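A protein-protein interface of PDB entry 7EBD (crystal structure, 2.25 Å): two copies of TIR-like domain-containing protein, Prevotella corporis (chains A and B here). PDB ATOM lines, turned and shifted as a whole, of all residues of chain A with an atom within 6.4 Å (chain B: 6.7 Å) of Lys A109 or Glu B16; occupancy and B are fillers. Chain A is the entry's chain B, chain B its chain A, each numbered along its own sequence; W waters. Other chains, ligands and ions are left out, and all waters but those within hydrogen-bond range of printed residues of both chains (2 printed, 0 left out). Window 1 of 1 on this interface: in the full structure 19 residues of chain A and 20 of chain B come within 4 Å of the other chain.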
ATOM      1  N   THR A  55      -6.963  27.595  30.285  1.00  0.00           N
ATOM      2  CA  THR A  55      -7.550  26.315  29.900  1.00  0.00           C
ATOM      3  C   THR A  55      -7.094  25.873  28.514  1.00  0.00           C
ATOM      4  O   THR A  55      -6.894  24.677  28.271  1.00  0.00           O
ATOM      5  CB  THR A  55      -9.076  26.401  29.955  1.00  0.00           C
ATOM      6  OG1 THR A  55      -9.527  27.450  29.088  1.00  0.00           O
ATOM      7  CG2 THR A  55      -9.540  26.689  31.374  1.00  0.00           C
ATOM      8  N   LYS A  58      -3.755  26.935  22.964  1.00  0.00           N
ATOM      9  CA  LYS A  58      -3.845  27.152  21.521  1.00  0.00           C
ATOM     10  C   LYS A  58      -4.615  28.426  21.196  1.00  0.00           C
ATOM     11  O   LYS A  58      -4.259  29.153  20.259  1.00  0.00           O
ATOM     12  CB  LYS A  58      -4.490  25.942  20.844  1.00  0.00           C
ATOM     13  CG  LYS A  58      -3.546  24.761  20.669  1.00  0.00           C
ATOM     14  CD  LYS A  58      -4.233  23.585  19.989  1.00  0.00           C
ATOM     15  CE  LYS A  58      -5.299  22.968  20.881  1.00  0.00           C
ATOM     16  NZ  LYS A  58      -5.831  21.695  20.313  1.00  0.00           N
ATOM     17  N   LEU A 104       2.886  23.086  26.723  1.00  0.00           N
ATOM     18  CA  LEU A 104       2.593  23.454  28.102  1.00  0.00           C
ATOM     19  C   LEU A 104       1.172  23.092  28.515  1.00  0.00           C
ATOM     20  O   LEU A 104       0.885  23.067  29.720  1.00  0.00           O
ATOM     21  CB  LEU A 104       2.820  24.952  28.304  1.00  0.00           C
ATOM     22  CG  LEU A 104       4.250  25.467  28.160  1.00  0.00           C
ATOM     23  CD1 LEU A 104       4.262  26.984  28.092  1.00  0.00           C
ATOM     24  CD2 LEU A 104       5.105  24.973  29.316  1.00  0.00           C
ATOM     25  N   SER A 105       0.290  22.806  27.552  1.00  0.00           N
ATOM     26  CA  SER A 105      -1.103  22.494  27.861  1.00  0.00           C
ATOM     27  C   SER A 105      -1.205  21.467  28.982  1.00  0.00           C
ATOM     28  O   SER A 105      -1.828  21.718  30.023  1.00  0.00           O
ATOM     29  CB  SER A 105      -1.812  21.991  26.602  1.00  0.00           C
ATOM     30  OG  SER A 105      -1.245  20.775  26.148  1.00  0.00           O
ATOM     31  N   GLY A 106      -0.558  20.314  28.796  1.00  0.00           N
ATOM     32  CA  GLY A 106      -0.596  19.270  29.809  1.00  0.00           C
ATOM     33  C   GLY A 106      -0.249  19.777  31.194  1.00  0.00           C
ATOM     34  O   GLY A 106      -0.948  19.478  32.168  1.00  0.00           O
ATOM     35  N   ILE A 107       0.818  20.580  31.290  1.00  0.00           N
ATOM     36  CA  ILE A 107       1.222  21.154  32.575  1.00  0.00           C
ATOM     37  C   ILE A 107       0.012  21.733  33.295  1.00  0.00           C
ATOM     38  O   ILE A 107      -0.306  21.344  34.427  1.00  0.00           O
ATOM     39  CB  ILE A 107       2.311  22.223  32.368  1.00  0.00           C
ATOM     40  CG1 ILE A 107       3.647  21.572  32.005  1.00  0.00           C
ATOM     41  CG2 ILE A 107       2.462  23.079  33.615  1.00  0.00           C
ATOM     42  CD1 ILE A 107       4.305  20.851  33.160  1.00  0.00           C
ATOM     43  N   ASP A 108      -0.713  22.625  32.614  1.00  0.00           N
ATOM     44  CA  ASP A 108      -1.905  23.233  33.194  1.00  0.00           C
ATOM     45  C   ASP A 108      -2.821  22.169  33.781  1.00  0.00           C
ATOM     46  O   ASP A 108      -3.117  22.173  34.983  1.00  0.00           O
ATOM     47  CB  ASP A 108      -2.636  24.054  32.132  1.00  0.00           C
ATOM     48  CG  ASP A 108      -1.714  24.999  31.395  1.00  0.00           C
ATOM     49  OD1 ASP A 108      -0.484  24.876  31.561  1.00  0.00           O
ATOM     50  OD2 ASP A 108      -2.217  25.866  30.650  1.00  0.00           O
ATOM     51  N   LYS A 109      -3.232  21.212  32.943  1.00  0.00           N
ATOM     52  CA  LYS A 109      -4.176  20.196  33.391  1.00  0.00           C
ATOM     53  C   LYS A 109      -3.630  19.435  34.590  1.00  0.00           C
ATOM     54  O   LYS A 109      -4.370  19.139  35.537  1.00  0.00           O
ATOM     55  CB  LYS A 109      -4.506  19.248  32.237  1.00  0.00           C
ATOM     56  CG  LYS A 109      -5.276  19.917  31.106  1.00  0.00           C
ATOM     57  CD  LYS A 109      -5.601  18.948  29.979  1.00  0.00           C
ATOM     58  CE  LYS A 109      -6.599  17.887  30.418  1.00  0.00           C
ATOM     59  NZ  LYS A 109      -6.979  16.987  29.292  1.00  0.00           N
ATOM     60  N   ALA A 110      -2.322  19.156  34.589  1.00  0.00           N
ATOM     61  CA  ALA A 110      -1.710  18.467  35.719  1.00  0.00           C
ATOM     62  C   ALA A 110      -1.949  19.232  37.012  1.00  0.00           C
ATOM     63  O   ALA A 110      -2.391  18.662  38.017  1.00  0.00           O
ATOM     64  CB  ALA A 110      -0.216  18.275  35.471  1.00  0.00           C
ATOM     65  N   ILE A 111      -1.683  20.540  36.991  1.00  0.00           N
ATOM     66  CA  ILE A 111      -1.907  21.363  38.174  1.00  0.00           C
ATOM     67  C   ILE A 111      -3.371  21.318  38.586  1.00  0.00           C
ATOM     68  O   ILE A 111      -3.690  21.340  39.782  1.00  0.00           O
ATOM     69  CB  ILE A 111      -1.423  22.801  37.910  1.00  0.00           C
ATOM     70  CG1 ILE A 111       0.075  22.794  37.600  1.00  0.00           C
ATOM     71  CG2 ILE A 111      -1.704  23.692  39.105  1.00  0.00           C
ATOM     72  CD1 ILE A 111       0.537  23.963  36.771  1.00  0.00           C
ATOM     73  N   ASP A 112      -4.283  21.235  37.615  1.00  0.00           N
ATOM     74  CA  ASP A 112      -5.703  21.178  37.939  1.00  0.00           C
ATOM     75  C   ASP A 112      -6.117  19.867  38.598  1.00  0.00           C
ATOM     76  O   ASP A 112      -7.306  19.698  38.889  1.00  0.00           O
ATOM     77  CB  ASP A 112      -6.538  21.411  36.680  1.00  0.00           C
ATOM     78  CG  ASP A 112      -6.352  22.801  36.109  1.00  0.00           C
ATOM     79  OD1 ASP A 112      -5.918  23.699  36.861  1.00  0.00           O
ATOM     80  OD2 ASP A 112      -6.640  22.998  34.910  1.00  0.00           O
ATOM     81  N   MET A 113      -5.191  18.944  38.842  1.00  0.00           N
ATOM     82  CA  MET A 113      -5.551  17.678  39.469  1.00  0.00           C
ATOM     83  C   MET A 113      -4.856  17.487  40.811  1.00  0.00           C
ATOM     84  O   MET A 113      -4.767  16.369  41.319  1.00  0.00           O
ATOM     85  CB  MET A 113      -5.223  16.509  38.542  1.00  0.00           C
ATOM     86  CG  MET A 113      -5.923  16.586  37.198  1.00  0.00           C
ATOM     87  SD  MET A 113      -5.887  14.889  36.251  1.00  0.00           S
ATOM     88  CE  MET A 113      -6.716  15.455  34.580  1.00  0.00           C
ATOM     89  N   TYR A 114      -4.363  18.582  41.387  1.00  0.00           N
ATOM     90  CA  TYR A 114      -3.721  18.507  42.693  1.00  0.00           C
ATOM     91  C   TYR A 114      -4.224  19.616  43.609  1.00  0.00           C
ATOM     92  O   TYR A 114      -4.297  19.430  44.828  1.00  0.00           O
ATOM     93  CB  TYR A 114      -2.200  18.578  42.533  1.00  0.00           C
ATOM     94  CG  TYR A 114      -1.408  18.214  43.771  1.00  0.00           C
ATOM     95  CD1 TYR A 114      -1.164  16.888  44.101  1.00  0.00           C
ATOM     96  CD2 TYR A 114      -0.898  19.198  44.601  1.00  0.00           C
ATOM     97  CE1 TYR A 114      -0.434  16.557  45.231  1.00  0.00           C
ATOM     98  CE2 TYR A 114      -0.170  18.880  45.728  1.00  0.00           C
ATOM     99  CZ  TYR A 114       0.060  17.560  46.039  1.00  0.00           C
ATOM    100  OH  TYR A 114       0.787  17.251  47.164  1.00  0.00           O
ATOM    101  N   ALA B  11       1.961  12.497  28.678  1.00  0.00           N
ATOM    102  CA  ALA B  11       0.802  11.842  28.082  1.00  0.00           C
ATOM    103  C   ALA B  11      -0.326  12.834  27.836  1.00  0.00           C
ATOM    104  O   ALA B  11      -0.986  12.784  26.792  1.00  0.00           O
ATOM    105  CB  ALA B  11       0.330  10.699  28.980  1.00  0.00           C
ATOM    106  N   ILE B  12      -0.555  13.749  28.781  1.00  0.00           N
ATOM    107  CA  ILE B  12      -1.620  14.735  28.604  1.00  0.00           C
ATOM    108  C   ILE B  12      -1.314  15.649  27.423  1.00  0.00           C
ATOM    109  O   ILE B  12      -2.195  15.945  26.604  1.00  0.00           O
ATOM    110  CB  ILE B  12      -1.836  15.538  29.898  1.00  0.00           C
ATOM    111  CG1 ILE B  12      -2.244  14.615  31.045  1.00  0.00           C
ATOM    112  CG2 ILE B  12      -2.905  16.591  29.686  1.00  0.00           C
ATOM    113  CD1 ILE B  12      -2.395  15.330  32.369  1.00  0.00           C
ATOM    114  N   SER B  13      -0.068  16.118  27.318  1.00  0.00           N
ATOM    115  CA  SER B  13       0.305  16.982  26.202  1.00  0.00           C
ATOM    116  C   SER B  13       0.200  16.245  24.874  1.00  0.00           C
ATOM    117  O   SER B  13      -0.276  16.806  23.880  1.00  0.00           O
ATOM    118  CB  SER B  13       1.724  17.520  26.400  1.00  0.00           C
ATOM    119  OG  SER B  13       1.769  18.476  27.442  1.00  0.00           O
ATOM    120  N   TYR B  14       0.624  14.980  24.843  1.00  0.00           N
ATOM    121  CA  TYR B  14       0.534  14.191  23.619  1.00  0.00           C
ATOM    122  C   TYR B  14      -0.915  13.969  23.209  1.00  0.00           C
ATOM    123  O   TYR B  14      -1.249  14.029  22.020  1.00  0.00           O
ATOM    124  CB  TYR B  14       1.259  12.859  23.820  1.00  0.00           C
ATOM    125  CG  TYR B  14       1.241  11.932  22.627  1.00  0.00           C
ATOM    126  CD1 TYR B  14       1.826  12.303  21.424  1.00  0.00           C
ATOM    127  CD2 TYR B  14       0.661  10.673  22.712  1.00  0.00           C
ATOM    128  CE1 TYR B  14       1.820  11.454  20.333  1.00  0.00           C
ATOM    129  CE2 TYR B  14       0.652   9.814  21.627  1.00  0.00           C
ATOM    130  CZ  TYR B  14       1.229  10.212  20.440  1.00  0.00           C
ATOM    131  OH  TYR B  14       1.222   9.364  19.356  1.00  0.00           O
ATOM    132  N   PHE B  15      -1.797  13.734  24.182  1.00  0.00           N
ATOM    133  CA  PHE B  15      -3.206  13.525  23.871  1.00  0.00           C
ATOM    134  C   PHE B  15      -3.863  14.812  23.387  1.00  0.00           C
ATOM    135  O   PHE B  15      -4.609  14.801  22.401  1.00  0.00           O
ATOM    136  CB  PHE B  15      -3.931  12.978  25.102  1.00  0.00           C
ATOM    137  CG  PHE B  15      -5.415  12.814  24.917  1.00  0.00           C
ATOM    138  CD1 PHE B  15      -5.931  11.675  24.322  1.00  0.00           C
ATOM    139  CD2 PHE B  15      -6.292  13.798  25.345  1.00  0.00           C
ATOM    140  CE1 PHE B  15      -7.295  11.524  24.153  1.00  0.00           C
ATOM    141  CE2 PHE B  15      -7.657  13.654  25.177  1.00  0.00           C
ATOM    142  CZ  PHE B  15      -8.159  12.515  24.581  1.00  0.00           C
ATOM    143  N   GLU B  16      -3.584  15.934  24.055  1.00  0.00           N
ATOM    144  CA  GLU B  16      -4.221  17.197  23.693  1.00  0.00           C
ATOM    145  C   GLU B  16      -3.709  17.723  22.358  1.00  0.00           C
ATOM    146  O   GLU B  16      -4.470  18.327  21.593  1.00  0.00           O
ATOM    147  CB  GLU B  16      -3.995  18.233  24.794  1.00  0.00           C
ATOM    148  CG  GLU B  16      -4.740  17.951  26.093  1.00  0.00           C
ATOM    149  CD  GLU B  16      -6.246  17.891  25.904  1.00  0.00           C
ATOM    150  OE1 GLU B  16      -6.874  16.938  26.410  1.00  0.00           O
ATOM    151  OE2 GLU B  16      -6.800  18.790  25.238  1.00  0.00           O
ATOM    152  N   GLY B  17      -2.430  17.515  22.062  1.00  0.00           N
ATOM    153  CA  GLY B  17      -1.831  18.071  20.870  1.00  0.00           C
ATOM    154  C   GLY B  17      -1.800  17.179  19.650  1.00  0.00           C
ATOM    155  O   GLY B  17      -1.341  17.623  18.595  1.00  0.00           O
ATOM    156  N   PHE B  18      -2.271  15.936  19.743  1.00  0.00           N
ATOM    157  CA  PHE B  18      -2.199  15.045  18.590  1.00  0.00           C
ATOM    158  C   PHE B  18      -3.305  13.997  18.570  1.00  0.00           C
ATOM    159  O   PHE B  18      -4.101  13.952  17.627  1.00  0.00           O
ATOM    160  CB  PHE B  18      -0.835  14.353  18.542  1.00  0.00           C
ATOM    161  CG  PHE B  18      -0.741  13.281  17.495  1.00  0.00           C
ATOM    162  CD1 PHE B  18      -0.657  13.612  16.153  1.00  0.00           C
ATOM    163  CD2 PHE B  18      -0.746  11.943  17.853  1.00  0.00           C
ATOM    164  CE1 PHE B  18      -0.576  12.627  15.184  1.00  0.00           C
ATOM    165  CE2 PHE B  18      -0.666  10.954  16.891  1.00  0.00           C
ATOM    166  CZ  PHE B  18      -0.581  11.295  15.555  1.00  0.00           C
ATOM    167  N   VAL B  19      -3.360  13.150  19.602  1.00  0.00           N
ATOM    168  CA  VAL B  19      -4.246  11.985  19.574  1.00  0.00           C
ATOM    169  C   VAL B  19      -5.700  12.416  19.440  1.00  0.00           C
ATOM    170  O   VAL B  19      -6.454  11.875  18.620  1.00  0.00           O
ATOM    171  CB  VAL B  19      -4.031  11.117  20.826  1.00  0.00           C
ATOM    172  CG1 VAL B  19      -5.017   9.957  20.840  1.00  0.00           C
ATOM    173  CG2 VAL B  19      -2.606  10.608  20.872  1.00  0.00           C
ATOM    174  N   LYS B  20      -6.121  13.385  20.254  1.00  0.00           N
ATOM    175  CA  LYS B  20      -7.508  13.841  20.215  1.00  0.00           C
ATOM    176  C   LYS B  20      -7.861  14.419  18.849  1.00  0.00           C
ATOM    177  O   LYS B  20      -8.905  14.091  18.271  1.00  0.00           O
ATOM    178  CB  LYS B  20      -7.744  14.865  21.327  1.00  0.00           C
ATOM    179  CG  LYS B  20      -9.180  15.338  21.458  1.00  0.00           C
ATOM    180  CD  LYS B  20      -9.372  16.140  22.737  1.00  0.00           C
ATOM    181  CE  LYS B  20      -8.454  17.351  22.782  1.00  0.00           C
ATOM    182  NZ  LYS B  20      -8.903  18.432  21.863  1.00  0.00           N
ATOM    183  N   LEU B  21      -6.986  15.271  18.309  1.00  0.00           N
ATOM    184  CA  LEU B  21      -7.246  15.883  17.011  1.00  0.00           C
ATOM    185  C   LEU B  21      -7.259  14.840  15.899  1.00  0.00           C
ATOM    186  O   LEU B  21      -8.098  14.901  14.991  1.00  0.00           O
ATOM    187  CB  LEU B  21      -6.195  16.955  16.723  1.00  0.00           C
ATOM    188  CG  LEU B  21      -5.895  17.957  17.839  1.00  0.00           C
ATOM    189  CD1 LEU B  21      -4.756  18.884  17.436  1.00  0.00           C
ATOM    190  CD2 LEU B  21      -7.140  18.753  18.203  1.00  0.00           C
ATOM    191  N   LEU B 144      -7.109   8.645  29.086  1.00  0.00           N
ATOM    192  CA  LEU B 144      -7.600   9.788  28.320  1.00  0.00           C
ATOM    193  C   LEU B 144      -8.343   9.338  27.068  1.00  0.00           C
ATOM    194  O   LEU B 144      -9.334   9.961  26.668  1.00  0.00           O
ATOM    195  CB  LEU B 144      -6.442  10.716  27.957  1.00  0.00           C
ATOM    196  CG  LEU B 144      -5.745  11.403  29.132  1.00  0.00           C
ATOM    197  CD1 LEU B 144      -4.549  12.210  28.654  1.00  0.00           C
ATOM    198  CD2 LEU B 144      -6.722  12.286  29.891  1.00  0.00           C
HETATM  199  O   HOH W   1      -0.606  19.777  23.690  1.00  0.00           O
HETATM  200  O   HOH W   2      -8.516  21.189  21.014  1.00  0.00           O
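The side-chain hydroxyl (OG) of Ser B13 sits at hydrogen-bond distance from the backbone NH (N) of Gly A106 (3.3 Å).
The side-chain carboxylate (OE1) of Glu B16 lies within salt-bridge range of the side-chain amino group (NZ) of Lys A109 (2.9 Å).
The side-chain amino group (NZ) of Lys B20 is in salt-bridge range of the side-chain carboxylate (OE2) of Glu B16, 3.99 Å away.
Lys A58 touches Glu B16.
Lys A58 touches Leu B21.
Ser A105 touches Glu B16.
Gly A106 touches Ile B12.
Ile B12 touches Lys A109.
Lys A109 touches just these residues of chain B: Ile B12 (3.6 Å) and Glu B16 (2.9 Å).
Of the printed residues of chain A, Glu B16 touches Lys A58, Ser A105 and Lys A109.
Printed residues of chain A within 4 Å of Ser B13: Gly A106 (3.3 Å).
Printed residues of chain A within 4 Å of Leu B21: Lys A58 (3.8 Å).
Of the printed residues of chain B, Lys A58 touches Glu B16 (3.9 Å) and Leu B21 (3.8 Å).
Printed residues of chain A within 4 Å of Ile B12: Gly A106 (3.5 Å) and Lys A109 (3.6 Å).
Printed residues of chain B within 4 Å of Gly A106: Ile B12 and Ser B13.
Thr A55 touches none of the printed residues of chain B.
The nearest printed residue of chain A that does not touch Glu B16 is Gly A106 (5.5 Å).
The nearest printed residue of chain B that does not touch Ser A105 is Ser B13 (4.01 Å).
Of the 12 printed residues of chain B, 4 touch a printed residue of chain A.
Hydrophobic or aromatic side chains of chain B within 4 Å of the printed part of chain A: Ile B12 and Leu B21.
Along chain B the printed residues that touch a printed residue of chain A span positions 12 to 21.
Among the printed residues, Asp or Glu carboxylates within 4 Å of a Lys or Arg side-chain nitrogen of the other chain: Lys A109 with Glu B16 (2.9 Å).
No position is printed for both chains.
Water W1 lies within hydrogen-bond range of the side-chain hydroxyl (OG) of Ser A105 (2.7 Å), the backbone carbonyl oxygen (O) of Ser B13 (3.0 Å) and the backbone NH (N) of Gly B17 (3.3 Å).
Water W2 lies within hydrogen-bond range of the side-chain amino group (NZ) of Lys A58 and the side-chain amino group (NZ) of Lys B20.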
